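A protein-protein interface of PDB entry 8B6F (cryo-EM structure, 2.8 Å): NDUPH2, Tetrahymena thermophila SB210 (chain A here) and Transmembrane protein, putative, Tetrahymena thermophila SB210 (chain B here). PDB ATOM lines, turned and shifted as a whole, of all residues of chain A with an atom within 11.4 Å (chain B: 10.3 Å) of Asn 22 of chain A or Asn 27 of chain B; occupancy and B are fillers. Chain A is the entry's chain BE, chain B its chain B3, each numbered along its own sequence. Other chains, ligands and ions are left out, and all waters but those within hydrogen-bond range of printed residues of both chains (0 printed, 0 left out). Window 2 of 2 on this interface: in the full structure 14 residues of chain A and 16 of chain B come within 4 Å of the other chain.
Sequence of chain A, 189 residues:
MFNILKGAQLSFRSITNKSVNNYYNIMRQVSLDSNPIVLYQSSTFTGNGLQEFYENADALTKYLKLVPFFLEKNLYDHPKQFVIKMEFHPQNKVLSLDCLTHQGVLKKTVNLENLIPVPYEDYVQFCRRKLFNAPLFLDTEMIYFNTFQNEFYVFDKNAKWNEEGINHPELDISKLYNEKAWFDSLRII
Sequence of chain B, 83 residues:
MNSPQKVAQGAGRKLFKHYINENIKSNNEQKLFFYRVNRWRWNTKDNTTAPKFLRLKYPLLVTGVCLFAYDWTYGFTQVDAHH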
ATOM      1  N   ASN A  22     -15.507   1.293 -26.050  1.00  0.00           N
ATOM      2  CA  ASN A  22     -16.605   1.083 -27.030  1.00  0.00           C
ATOM      3  C   ASN A  22     -16.044   1.025 -28.443  1.00  0.00           C
ATOM      4  O   ASN A  22     -15.628   2.042 -28.998  1.00  0.00           O
ATOM      5  CB  ASN A  22     -17.643   2.200 -26.920  1.00  0.00           C
ATOM      6  CG  ASN A  22     -18.243   2.301 -25.531  1.00  0.00           C
ATOM      7  OD1 ASN A  22     -17.788   3.088 -24.701  1.00  0.00           O
ATOM      8  ND2 ASN A  22     -19.266   1.495 -25.271  1.00  0.00           N
ATOM      9  N   TYR A  23     -16.034  -0.171 -29.020  1.00  0.00           N
ATOM     10  CA  TYR A  23     -15.568  -0.393 -30.381  1.00  0.00           C
ATOM     11  C   TYR A  23     -16.774  -0.626 -31.278  1.00  0.00           C
ATOM     12  O   TYR A  23     -17.616  -1.479 -30.980  1.00  0.00           O
ATOM     13  CB  TYR A  23     -14.612  -1.585 -30.448  1.00  0.00           C
ATOM     14  CG  TYR A  23     -13.869  -1.694 -31.759  1.00  0.00           C
ATOM     15  CD1 TYR A  23     -14.432  -2.347 -32.849  1.00  0.00           C
ATOM     16  CD2 TYR A  23     -12.600  -1.148 -31.904  1.00  0.00           C
ATOM     17  CE1 TYR A  23     -13.753  -2.448 -34.049  1.00  0.00           C
ATOM     18  CE2 TYR A  23     -11.913  -1.244 -33.100  1.00  0.00           C
ATOM     19  CZ  TYR A  23     -12.494  -1.895 -34.168  1.00  0.00           C
ATOM     20  OH  TYR A  23     -11.811  -1.993 -35.358  1.00  0.00           O
ATOM     21  N   TYR A  24     -16.854   0.129 -32.369  1.00  0.00           N
ATOM     22  CA  TYR A  24     -17.985   0.083 -33.283  1.00  0.00           C
ATOM     23  C   TYR A  24     -17.554  -0.495 -34.621  1.00  0.00           C
ATOM     24  O   TYR A  24     -16.455  -0.210 -35.107  1.00  0.00           O
ATOM     25  CB  TYR A  24     -18.576   1.477 -33.484  1.00  0.00           C
ATOM     26  CG  TYR A  24     -19.042   2.113 -32.200  1.00  0.00           C
ATOM     27  CD1 TYR A  24     -20.337   1.925 -31.739  1.00  0.00           C
ATOM     28  CD2 TYR A  24     -18.184   2.894 -31.444  1.00  0.00           C
ATOM     29  CE1 TYR A  24     -20.763   2.503 -30.563  1.00  0.00           C
ATOM     30  CE2 TYR A  24     -18.599   3.475 -30.270  1.00  0.00           C
ATOM     31  CZ  TYR A  24     -19.887   3.274 -29.834  1.00  0.00           C
ATOM     32  OH  TYR A  24     -20.289   3.860 -28.664  1.00  0.00           O
ATOM     33  N   ASN A  25     -18.426  -1.312 -35.211  1.00  0.00           N
ATOM     34  CA  ASN A  25     -18.127  -1.995 -36.468  1.00  0.00           C
ATOM     35  C   ASN A  25     -18.475  -1.066 -37.628  1.00  0.00           C
ATOM     36  O   ASN A  25     -19.551  -1.129 -38.223  1.00  0.00           O
ATOM     37  CB  ASN A  25     -18.890  -3.312 -36.552  1.00  0.00           C
ATOM     38  CG  ASN A  25     -18.653  -4.199 -35.350  1.00  0.00           C
ATOM     39  OD1 ASN A  25     -18.329  -3.720 -34.266  1.00  0.00           O
ATOM     40  ND2 ASN A  25     -18.807  -5.502 -35.538  1.00  0.00           N
ATOM     41  N   ILE A  26     -17.535  -0.184 -37.948  1.00  0.00           N
ATOM     42  CA  ILE A  26     -17.679   0.735 -39.071  1.00  0.00           C
ATOM     43  C   ILE A  26     -17.029   0.103 -40.294  1.00  0.00           C
ATOM     44  O   ILE A  26     -15.872  -0.331 -40.241  1.00  0.00           O
ATOM     45  CB  ILE A  26     -17.051   2.101 -38.749  1.00  0.00           C
ATOM     46  CG1 ILE A  26     -17.698   2.689 -37.491  1.00  0.00           C
ATOM     47  CG2 ILE A  26     -17.209   3.048 -39.934  1.00  0.00           C
ATOM     48  CD1 ILE A  26     -17.107   4.011 -37.042  1.00  0.00           C
ATOM     49  N   THR A 147     -12.718 -10.170 -35.517  1.00  0.00           N
ATOM     50  CA  THR A 147     -13.561  -9.491 -34.542  1.00  0.00           C
ATOM     51  C   THR A 147     -14.791  -8.868 -35.185  1.00  0.00           C
ATOM     52  O   THR A 147     -15.847  -8.798 -34.547  1.00  0.00           O
ATOM     53  CB  THR A 147     -12.761  -8.414 -33.808  1.00  0.00           C
ATOM     54  OG1 THR A 147     -12.255  -7.460 -34.750  1.00  0.00           O
ATOM     55  CG2 THR A 147     -11.603  -9.032 -33.045  1.00  0.00           C
ATOM     56  N   ASN A 178      -1.646  -4.290 -31.996  1.00  0.00           N
ATOM     57  CA  ASN A 178      -2.409  -3.399 -31.127  1.00  0.00           C
ATOM     58  C   ASN A 178      -2.657  -4.153 -29.830  1.00  0.00           C
ATOM     59  O   ASN A 178      -3.376  -5.155 -29.825  1.00  0.00           O
ATOM     60  CB  ASN A 178      -3.718  -2.972 -31.785  1.00  0.00           C
ATOM     61  CG  ASN A 178      -4.501  -1.992 -30.938  1.00  0.00           C
ATOM     62  OD1 ASN A 178      -5.409  -2.377 -30.202  1.00  0.00           O
ATOM     63  ND2 ASN A 178      -4.153  -0.714 -31.036  1.00  0.00           N
ATOM     64  N   GLU A 179      -2.061  -3.676 -28.735  1.00  0.00           N
ATOM     65  CA  GLU A 179      -2.149  -4.405 -27.474  1.00  0.00           C
ATOM     66  C   GLU A 179      -3.593  -4.536 -27.014  1.00  0.00           C
ATOM     67  O   GLU A 179      -4.044  -5.627 -26.648  1.00  0.00           O
ATOM     68  CB  GLU A 179      -1.307  -3.704 -26.408  1.00  0.00           C
ATOM     69  CG  GLU A 179      -1.295  -4.421 -25.068  1.00  0.00           C
ATOM     70  CD  GLU A 179      -0.484  -3.683 -24.025  1.00  0.00           C
ATOM     71  OE1 GLU A 179       0.096  -2.629 -24.358  1.00  0.00           O
ATOM     72  OE2 GLU A 179      -0.425  -4.158 -22.872  1.00  0.00           O
ATOM     73  N   LYS A 180      -4.337  -3.430 -27.024  1.00  0.00           N
ATOM     74  CA  LYS A 180      -5.700  -3.458 -26.507  1.00  0.00           C
ATOM     75  C   LYS A 180      -6.578  -4.398 -27.324  1.00  0.00           C
ATOM     76  O   LYS A 180      -7.407  -5.126 -26.768  1.00  0.00           O
ATOM     77  CB  LYS A 180      -6.282  -2.046 -26.497  1.00  0.00           C
ATOM     78  CG  LYS A 180      -7.445  -1.869 -25.534  1.00  0.00           C
ATOM     79  CD  LYS A 180      -7.907  -0.422 -25.485  1.00  0.00           C
ATOM     80  CE  LYS A 180      -8.906  -0.197 -24.361  1.00  0.00           C
ATOM     81  NZ  LYS A 180     -10.098  -1.081 -24.480  1.00  0.00           N
ATOM     82  N   ALA A 181      -6.414  -4.391 -28.647  1.00  0.00           N
ATOM     83  CA  ALA A 181      -7.233  -5.251 -29.495  1.00  0.00           C
ATOM     84  C   ALA A 181      -6.828  -6.715 -29.368  1.00  0.00           C
ATOM     85  O   ALA A 181      -7.688  -7.596 -29.262  1.00  0.00           O
ATOM     86  CB  ALA A 181      -7.136  -4.796 -30.950  1.00  0.00           C
ATOM     87  N   TRP A 182      -5.525  -7.000 -29.378  1.00  0.00           N
ATOM     88  CA  TRP A 182      -5.082  -8.391 -29.396  1.00  0.00           C
ATOM     89  C   TRP A 182      -5.291  -9.069 -28.048  1.00  0.00           C
ATOM     90  O   TRP A 182      -5.650 -10.250 -27.995  1.00  0.00           O
ATOM     91  CB  TRP A 182      -3.612  -8.471 -29.810  1.00  0.00           C
ATOM     92  CG  TRP A 182      -3.394  -8.284 -31.280  1.00  0.00           C
ATOM     93  CD1 TRP A 182      -4.266  -7.739 -32.175  1.00  0.00           C
ATOM     94  CD2 TRP A 182      -2.230  -8.654 -32.028  1.00  0.00           C
ATOM     95  NE1 TRP A 182      -3.716  -7.744 -33.434  1.00  0.00           N
ATOM     96  CE2 TRP A 182      -2.467  -8.298 -33.370  1.00  0.00           C
ATOM     97  CE3 TRP A 182      -1.009  -9.248 -31.690  1.00  0.00           C
ATOM     98  CZ2 TRP A 182      -1.528  -8.517 -34.376  1.00  0.00           C
ATOM     99  CZ3 TRP A 182      -0.077  -9.465 -32.691  1.00  0.00           C
ATOM    100  CH2 TRP A 182      -0.342  -9.100 -34.018  1.00  0.00           C
ATOM    101  N   ASP A 184      -7.145  -7.670 -25.154  1.00  0.00           N
ATOM    102  CA  ASP A 184      -8.319  -7.317 -24.368  1.00  0.00           C
ATOM    103  C   ASP A 184      -9.615  -7.313 -25.165  1.00  0.00           C
ATOM    104  O   ASP A 184     -10.678  -7.082 -24.579  1.00  0.00           O
ATOM    105  CB  ASP A 184      -8.124  -5.938 -23.723  1.00  0.00           C
ATOM    106  CG  ASP A 184      -6.868  -5.864 -22.877  1.00  0.00           C
ATOM    107  OD1 ASP A 184      -6.527  -6.875 -22.231  1.00  0.00           O
ATOM    108  OD2 ASP A 184      -6.220  -4.796 -22.862  1.00  0.00           O
ATOM    109  N   SER A 185      -9.568  -7.557 -26.475  1.00  0.00           N
ATOM    110  CA  SER A 185     -10.794  -7.514 -27.264  1.00  0.00           C
ATOM    111  C   SER A 185     -11.684  -8.717 -26.977  1.00  0.00           C
ATOM    112  O   SER A 185     -12.899  -8.569 -26.808  1.00  0.00           O
ATOM    113  CB  SER A 185     -10.457  -7.445 -28.752  1.00  0.00           C
ATOM    114  OG  SER A 185     -11.632  -7.344 -29.539  1.00  0.00           O
ATOM    115  N   LEU A 186     -11.102  -9.911 -26.916  1.00  0.00           N
ATOM    116  CA  LEU A 186     -11.852 -11.151 -26.730  1.00  0.00           C
ATOM    117  C   LEU A 186     -11.578 -11.667 -25.322  1.00  0.00           C
ATOM    118  O   LEU A 186     -10.513 -12.229 -25.053  1.00  0.00           O
ATOM    119  CB  LEU A 186     -11.468 -12.181 -27.789  1.00  0.00           C
ATOM    120  CG  LEU A 186     -12.242 -13.501 -27.763  1.00  0.00           C
ATOM    121  CD1 LEU A 186     -13.720 -13.271 -28.021  1.00  0.00           C
ATOM    122  CD2 LEU A 186     -11.670 -14.474 -28.777  1.00  0.00           C
ATOM    123  N   TYR B  19     -21.128  11.357 -31.378  1.00  0.00           N
ATOM    124  CA  TYR B  19     -21.128  10.634 -30.113  1.00  0.00           C
ATOM    125  C   TYR B  19     -20.374   9.314 -30.202  1.00  0.00           C
ATOM    126  O   TYR B  19     -19.846   8.841 -29.190  1.00  0.00           O
ATOM    127  CB  TYR B  19     -22.562  10.416 -29.639  1.00  0.00           C
ATOM    128  CG  TYR B  19     -23.199  11.703 -29.173  1.00  0.00           C
ATOM    129  CD1 TYR B  19     -22.861  12.261 -27.947  1.00  0.00           C
ATOM    130  CD2 TYR B  19     -24.118  12.370 -29.966  1.00  0.00           C
ATOM    131  CE1 TYR B  19     -23.431  13.443 -27.521  1.00  0.00           C
ATOM    132  CE2 TYR B  19     -24.693  13.552 -29.550  1.00  0.00           C
ATOM    133  CZ  TYR B  19     -24.346  14.083 -28.326  1.00  0.00           C
ATOM    134  OH  TYR B  19     -24.920  15.260 -27.908  1.00  0.00           O
ATOM    135  N   ILE B  20     -20.303   8.711 -31.389  1.00  0.00           N
ATOM    136  CA  ILE B  20     -19.438   7.549 -31.565  1.00  0.00           C
ATOM    137  C   ILE B  20     -17.984   7.946 -31.356  1.00  0.00           C
ATOM    138  O   ILE B  20     -17.220   7.237 -30.692  1.00  0.00           O
ATOM    139  CB  ILE B  20     -19.666   6.916 -32.953  1.00  0.00           C
ATOM    140  CG1 ILE B  20     -21.005   6.177 -32.980  1.00  0.00           C
ATOM    141  CG2 ILE B  20     -18.524   5.975 -33.324  1.00  0.00           C
ATOM    142  CD1 ILE B  20     -21.466   5.794 -34.367  1.00  0.00           C
ATOM    143  N   ASN B  21     -17.581   9.087 -31.914  1.00  0.00           N
ATOM    144  CA  ASN B  21     -16.225   9.574 -31.689  1.00  0.00           C
ATOM    145  C   ASN B  21     -15.995   9.880 -30.215  1.00  0.00           C
ATOM    146  O   ASN B  21     -14.921   9.594 -29.674  1.00  0.00           O
ATOM    147  CB  ASN B  21     -15.968  10.813 -32.543  1.00  0.00           C
ATOM    148  CG  ASN B  21     -15.975  10.506 -34.025  1.00  0.00           C
ATOM    149  OD1 ASN B  21     -16.428   9.443 -34.446  1.00  0.00           O
ATOM    150  ND2 ASN B  21     -15.476  11.439 -34.825  1.00  0.00           N
ATOM    151  N   GLU B  22     -16.993  10.462 -29.547  1.00  0.00           N
ATOM    152  CA  GLU B  22     -16.861  10.734 -28.120  1.00  0.00           C
ATOM    153  C   GLU B  22     -16.665   9.448 -27.328  1.00  0.00           C
ATOM    154  O   GLU B  22     -15.813   9.385 -26.434  1.00  0.00           O
ATOM    155  CB  GLU B  22     -18.095  11.483 -27.617  1.00  0.00           C
ATOM    156  CG  GLU B  22     -18.206  12.908 -28.128  1.00  0.00           C
ATOM    157  CD  GLU B  22     -17.109  13.803 -27.593  1.00  0.00           C
ATOM    158  OE1 GLU B  22     -16.428  13.398 -26.628  1.00  0.00           O
ATOM    159  OE2 GLU B  22     -16.927  14.912 -28.137  1.00  0.00           O
ATOM    160  N   ASN B  23     -17.445   8.411 -27.638  1.00  0.00           N
ATOM    161  CA  ASN B  23     -17.296   7.142 -26.932  1.00  0.00           C
ATOM    162  C   ASN B  23     -15.940   6.507 -27.214  1.00  0.00           C
ATOM    163  O   ASN B  23     -15.320   5.928 -26.316  1.00  0.00           O
ATOM    164  CB  ASN B  23     -18.431   6.194 -27.317  1.00  0.00           C
ATOM    165  CG  ASN B  23     -19.789   6.708 -26.878  1.00  0.00           C
ATOM    166  OD1 ASN B  23     -19.931   7.875 -26.515  1.00  0.00           O
ATOM    167  ND2 ASN B  23     -20.794   5.840 -26.901  1.00  0.00           N
ATOM    168  N   ILE B  24     -15.468   6.597 -28.459  1.00  0.00           N
ATOM    169  CA  ILE B  24     -14.150   6.061 -28.794  1.00  0.00           C
ATOM    170  C   ILE B  24     -13.070   6.788 -28.007  1.00  0.00           C
ATOM    171  O   ILE B  24     -12.135   6.171 -27.485  1.00  0.00           O
ATOM    172  CB  ILE B  24     -13.907   6.151 -30.313  1.00  0.00           C
ATOM    173  CG1 ILE B  24     -14.849   5.204 -31.056  1.00  0.00           C
ATOM    174  CG2 ILE B  24     -12.456   5.825 -30.650  1.00  0.00           C
ATOM    175  CD1 ILE B  24     -14.890   5.430 -32.553  1.00  0.00           C
ATOM    176  N   LYS B  25     -13.180   8.114 -27.913  1.00  0.00           N
ATOM    177  CA  LYS B  25     -12.218   8.884 -27.135  1.00  0.00           C
ATOM    178  C   LYS B  25     -12.262   8.489 -25.666  1.00  0.00           C
ATOM    179  O   LYS B  25     -11.216   8.330 -25.025  1.00  0.00           O
ATOM    180  CB  LYS B  25     -12.502  10.377 -27.297  1.00  0.00           C
ATOM    181  CG  LYS B  25     -11.471  11.288 -26.652  1.00  0.00           C
ATOM    182  CD  LYS B  25     -11.986  12.718 -26.548  1.00  0.00           C
ATOM    183  CE  LYS B  25     -12.354  13.287 -27.912  1.00  0.00           C
ATOM    184  NZ  LYS B  25     -12.822  14.698 -27.813  1.00  0.00           N
ATOM    185  N   SER B  26     -13.464   8.322 -25.114  1.00  0.00           N
ATOM    186  CA  SER B  26     -13.585   7.927 -23.715  1.00  0.00           C
ATOM    187  C   SER B  26     -12.942   6.568 -23.471  1.00  0.00           C
ATOM    188  O   SER B  26     -12.244   6.373 -22.470  1.00  0.00           O
ATOM    189  CB  SER B  26     -15.058   7.903 -23.307  1.00  0.00           C
ATOM    190  OG  SER B  26     -15.206   7.570 -21.940  1.00  0.00           O
ATOM    191  N   ASN B  27     -13.167   5.616 -24.377  1.00  0.00           N
ATOM    192  CA  ASN B  27     -12.550   4.301 -24.242  1.00  0.00           C
ATOM    193  C   ASN B  27     -11.033   4.389 -24.353  1.00  0.00           C
ATOM    194  O   ASN B  27     -10.309   3.726 -23.603  1.00  0.00           O
ATOM    195  CB  ASN B  27     -13.111   3.352 -25.298  1.00  0.00           C
ATOM    196  CG  ASN B  27     -12.613   1.931 -25.127  1.00  0.00           C
ATOM    197  OD1 ASN B  27     -12.289   1.503 -24.021  1.00  0.00           O
ATOM    198  ND2 ASN B  27     -12.546   1.190 -26.227  1.00  0.00           N
ATOM    199  N   ASN B  28     -10.532   5.204 -25.284  1.00  0.00           N
ATOM    200  CA  ASN B  28      -9.087   5.339 -25.445  1.00  0.00           C
ATOM    201  C   ASN B  28      -8.436   5.968 -24.221  1.00  0.00           C
ATOM    202  O   ASN B  28      -7.264   5.695 -23.938  1.00  0.00           O
ATOM    203  CB  ASN B  28      -8.775   6.173 -26.687  1.00  0.00           C
ATOM    204  CG  ASN B  28      -9.259   5.519 -27.961  1.00  0.00           C
ATOM    205  OD1 ASN B  28      -9.321   4.295 -28.060  1.00  0.00           O
ATOM    206  ND2 ASN B  28      -9.603   6.335 -28.950  1.00  0.00           N
ATOM    207  N   GLU B  29      -9.166   6.808 -23.490  1.00  0.00           N
ATOM    208  CA  GLU B  29      -8.610   7.450 -22.306  1.00  0.00           C
ATOM    209  C   GLU B  29      -8.317   6.465 -21.183  1.00  0.00           C
ATOM    210  O   GLU B  29      -7.654   6.844 -20.213  1.00  0.00           O
ATOM    211  CB  GLU B  29      -9.558   8.539 -21.801  1.00  0.00           C
ATOM    212  CG  GLU B  29      -9.505   9.823 -22.615  1.00  0.00           C
ATOM    213  CD  GLU B  29     -10.398  10.910 -22.050  1.00  0.00           C
ATOM    214  OE1 GLU B  29     -11.072  10.656 -21.030  1.00  0.00           O
ATOM    215  OE2 GLU B  29     -10.426  12.018 -22.626  1.00  0.00           O
ATOM    216  N   GLN B  30      -8.787   5.225 -21.283  1.00  0.00           N
ATOM    217  CA  GLN B  30      -8.537   4.251 -20.236  1.00  0.00           C
ATOM    218  C   GLN B  30      -7.052   3.905 -20.160  1.00  0.00           C
ATOM    219  O   GLN B  30      -6.301   4.040 -21.129  1.00  0.00           O
ATOM    220  CB  GLN B  30      -9.341   2.974 -20.488  1.00  0.00           C
ATOM    221  CG  GLN B  30     -10.838   3.134 -20.298  1.00  0.00           C
ATOM    222  CD  GLN B  30     -11.588   1.829 -20.420  1.00  0.00           C
ATOM    223  OE1 GLN B  30     -11.022   0.803 -20.793  1.00  0.00           O
ATOM    224  NE2 GLN B  30     -12.871   1.855 -20.079  1.00  0.00           N
ATOM    225  N   LYS B  31      -6.633   3.457 -18.979  1.00  0.00           N
ATOM    226  CA  LYS B  31      -5.260   3.033 -18.741  1.00  0.00           C
ATOM    227  C   LYS B  31      -5.143   1.525 -18.911  1.00  0.00           C
ATOM    228  O   LYS B  31      -5.994   0.768 -18.440  1.00  0.00           O
ATOM    229  CB  LYS B  31      -4.794   3.429 -17.337  1.00  0.00           C
ATOM    230  CG  LYS B  31      -4.754   4.926 -17.087  1.00  0.00           C
ATOM    231  CD  LYS B  31      -4.194   5.234 -15.707  1.00  0.00           C
ATOM    232  CE  LYS B  31      -4.201   6.727 -15.421  1.00  0.00           C
ATOM    233  NZ  LYS B  31      -5.580   7.283 -15.363  1.00  0.00           N
ATOM    234  N   LEU B  32      -4.078   1.095 -19.584  1.00  0.00           N
ATOM    235  CA  LEU B  32      -3.830  -0.324 -19.800  1.00  0.00           C
ATOM    236  C   LEU B  32      -3.182  -0.995 -18.599  1.00  0.00           C
ATOM    237  O   LEU B  32      -3.003  -2.217 -18.614  1.00  0.00           O
ATOM    238  CB  LEU B  32      -2.950  -0.520 -21.035  1.00  0.00           C
ATOM    239  CG  LEU B  32      -3.526  -0.013 -22.358  1.00  0.00           C
ATOM    240  CD1 LEU B  32      -2.523  -0.214 -23.478  1.00  0.00           C
ATOM    241  CD2 LEU B  32      -4.841  -0.705 -22.688  1.00  0.00           C
ATOM    242  N   TYR B  35      -5.679  -3.494 -17.063  1.00  0.00           N
ATOM    243  CA  TYR B  35      -5.796  -4.658 -17.935  1.00  0.00           C
ATOM    244  C   TYR B  35      -4.584  -5.567 -17.797  1.00  0.00           C
ATOM    245  O   TYR B  35      -4.719  -6.788 -17.667  1.00  0.00           O
ATOM    246  CB  TYR B  35      -5.957  -4.216 -19.388  1.00  0.00           C
ATOM    247  CG  TYR B  35      -7.278  -3.557 -19.696  1.00  0.00           C
ATOM    248  CD1 TYR B  35      -8.373  -4.309 -20.095  1.00  0.00           C
ATOM    249  CD2 TYR B  35      -7.424  -2.181 -19.607  1.00  0.00           C
ATOM    250  CE1 TYR B  35      -9.579  -3.713 -20.385  1.00  0.00           C
ATOM    251  CE2 TYR B  35      -8.626  -1.574 -19.895  1.00  0.00           C
ATOM    252  CZ  TYR B  35      -9.700  -2.345 -20.285  1.00  0.00           C
ATOM    253  OH  TYR B  35     -10.902  -1.745 -20.572  1.00  0.00           O
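Of chain B, only Ile 24 (3.9 Å) and Asn 27 (3.0 Å) come within 4 Å of Asn 22 of chain A. Printed residues of chain B within 4 Å of Lys 180 of chain A: Asn 27. Of the printed residues of chain B, Asp 184 of chain A touches Tyr 35. Printed residues of chain A within 4 Å of Ile 20 of chain B: Tyr 24 (3.6 Å). Of the printed residues of chain A, Asn 23 of chain B touches Tyr 24 (2.7 Å). Ile 24 of chain B touches just one residue of chain A: Asn 22. Of chain A, only Asn 22 (3.0 Å) and Lys 180 (3.4 Å) come within 4 Å of Asn 27 of chain B. No residue of chain A comes within 4 Å of Asn 28 of chain B. No residue of chain A comes within 4 Å of Glu 29 of chain B. No residue of chain A comes within 4 Å of Gln 30 of chain B. Of the printed residues of chain A, Tyr 35 of chain B touches Asp 184 (3.5 Å). The nearest residue of chain B that does not touch Asn 22 of chain A is Asn 23 of chain B (4.1 Å).
The side-chain hydroxyl (OH) of Tyr 24 of chain A is in hydrogen-bond range of the side-chain amide nitrogen (ND2) of Asn 23 of chain B, at 2.7 Å. The side-chain amide oxygen (OD1) of Asn 27 of chain B lies within hydrogen-bond range of the side-chain amino group (NZ) of Lys 180 of chain A, 3.4 Å away. The backbone NH (N) of Asn 22 of chain A lies close to the side-chain amide nitrogen (ND2) of Asn 27 of chain B (3.0 Å).
The side-chain amide oxygen of Asn 23 of chain B lies close to the backbone carbonyl oxygen of Tyr 19 of chain B (2.8 Å). The side-chain amide oxygen (OE1) of Gln 30 of chain B sits at hydrogen-bond distance from the side-chain hydroxyl (OH) of Tyr 35 of chain B (2.6 Å). O of Lys 180 of chain A lies within hydrogen-bond range of N of Ser 185 of chain A (3.3 Å). The side-chain amide nitrogen (ND2) of Asn 28 of chain B lies within hydrogen-bond range of the backbone carbonyl oxygen (O) of Ile 24 of chain B (2.9 Å).
Among the printed residues, merely in contact across the chains: Asp 184 of chain A with Tyr 35 of chain B (3.5 Å), Tyr 24 of chain A with Ile 20 of chain B (3.6 Å), Glu 179 of chain A with Leu 32 of chain B (3.7 Å) and Asn 22 of chain A with Ile 24 of chain B (3.9 Å).
Among the printed residues, 7 pairs touch across the chains.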
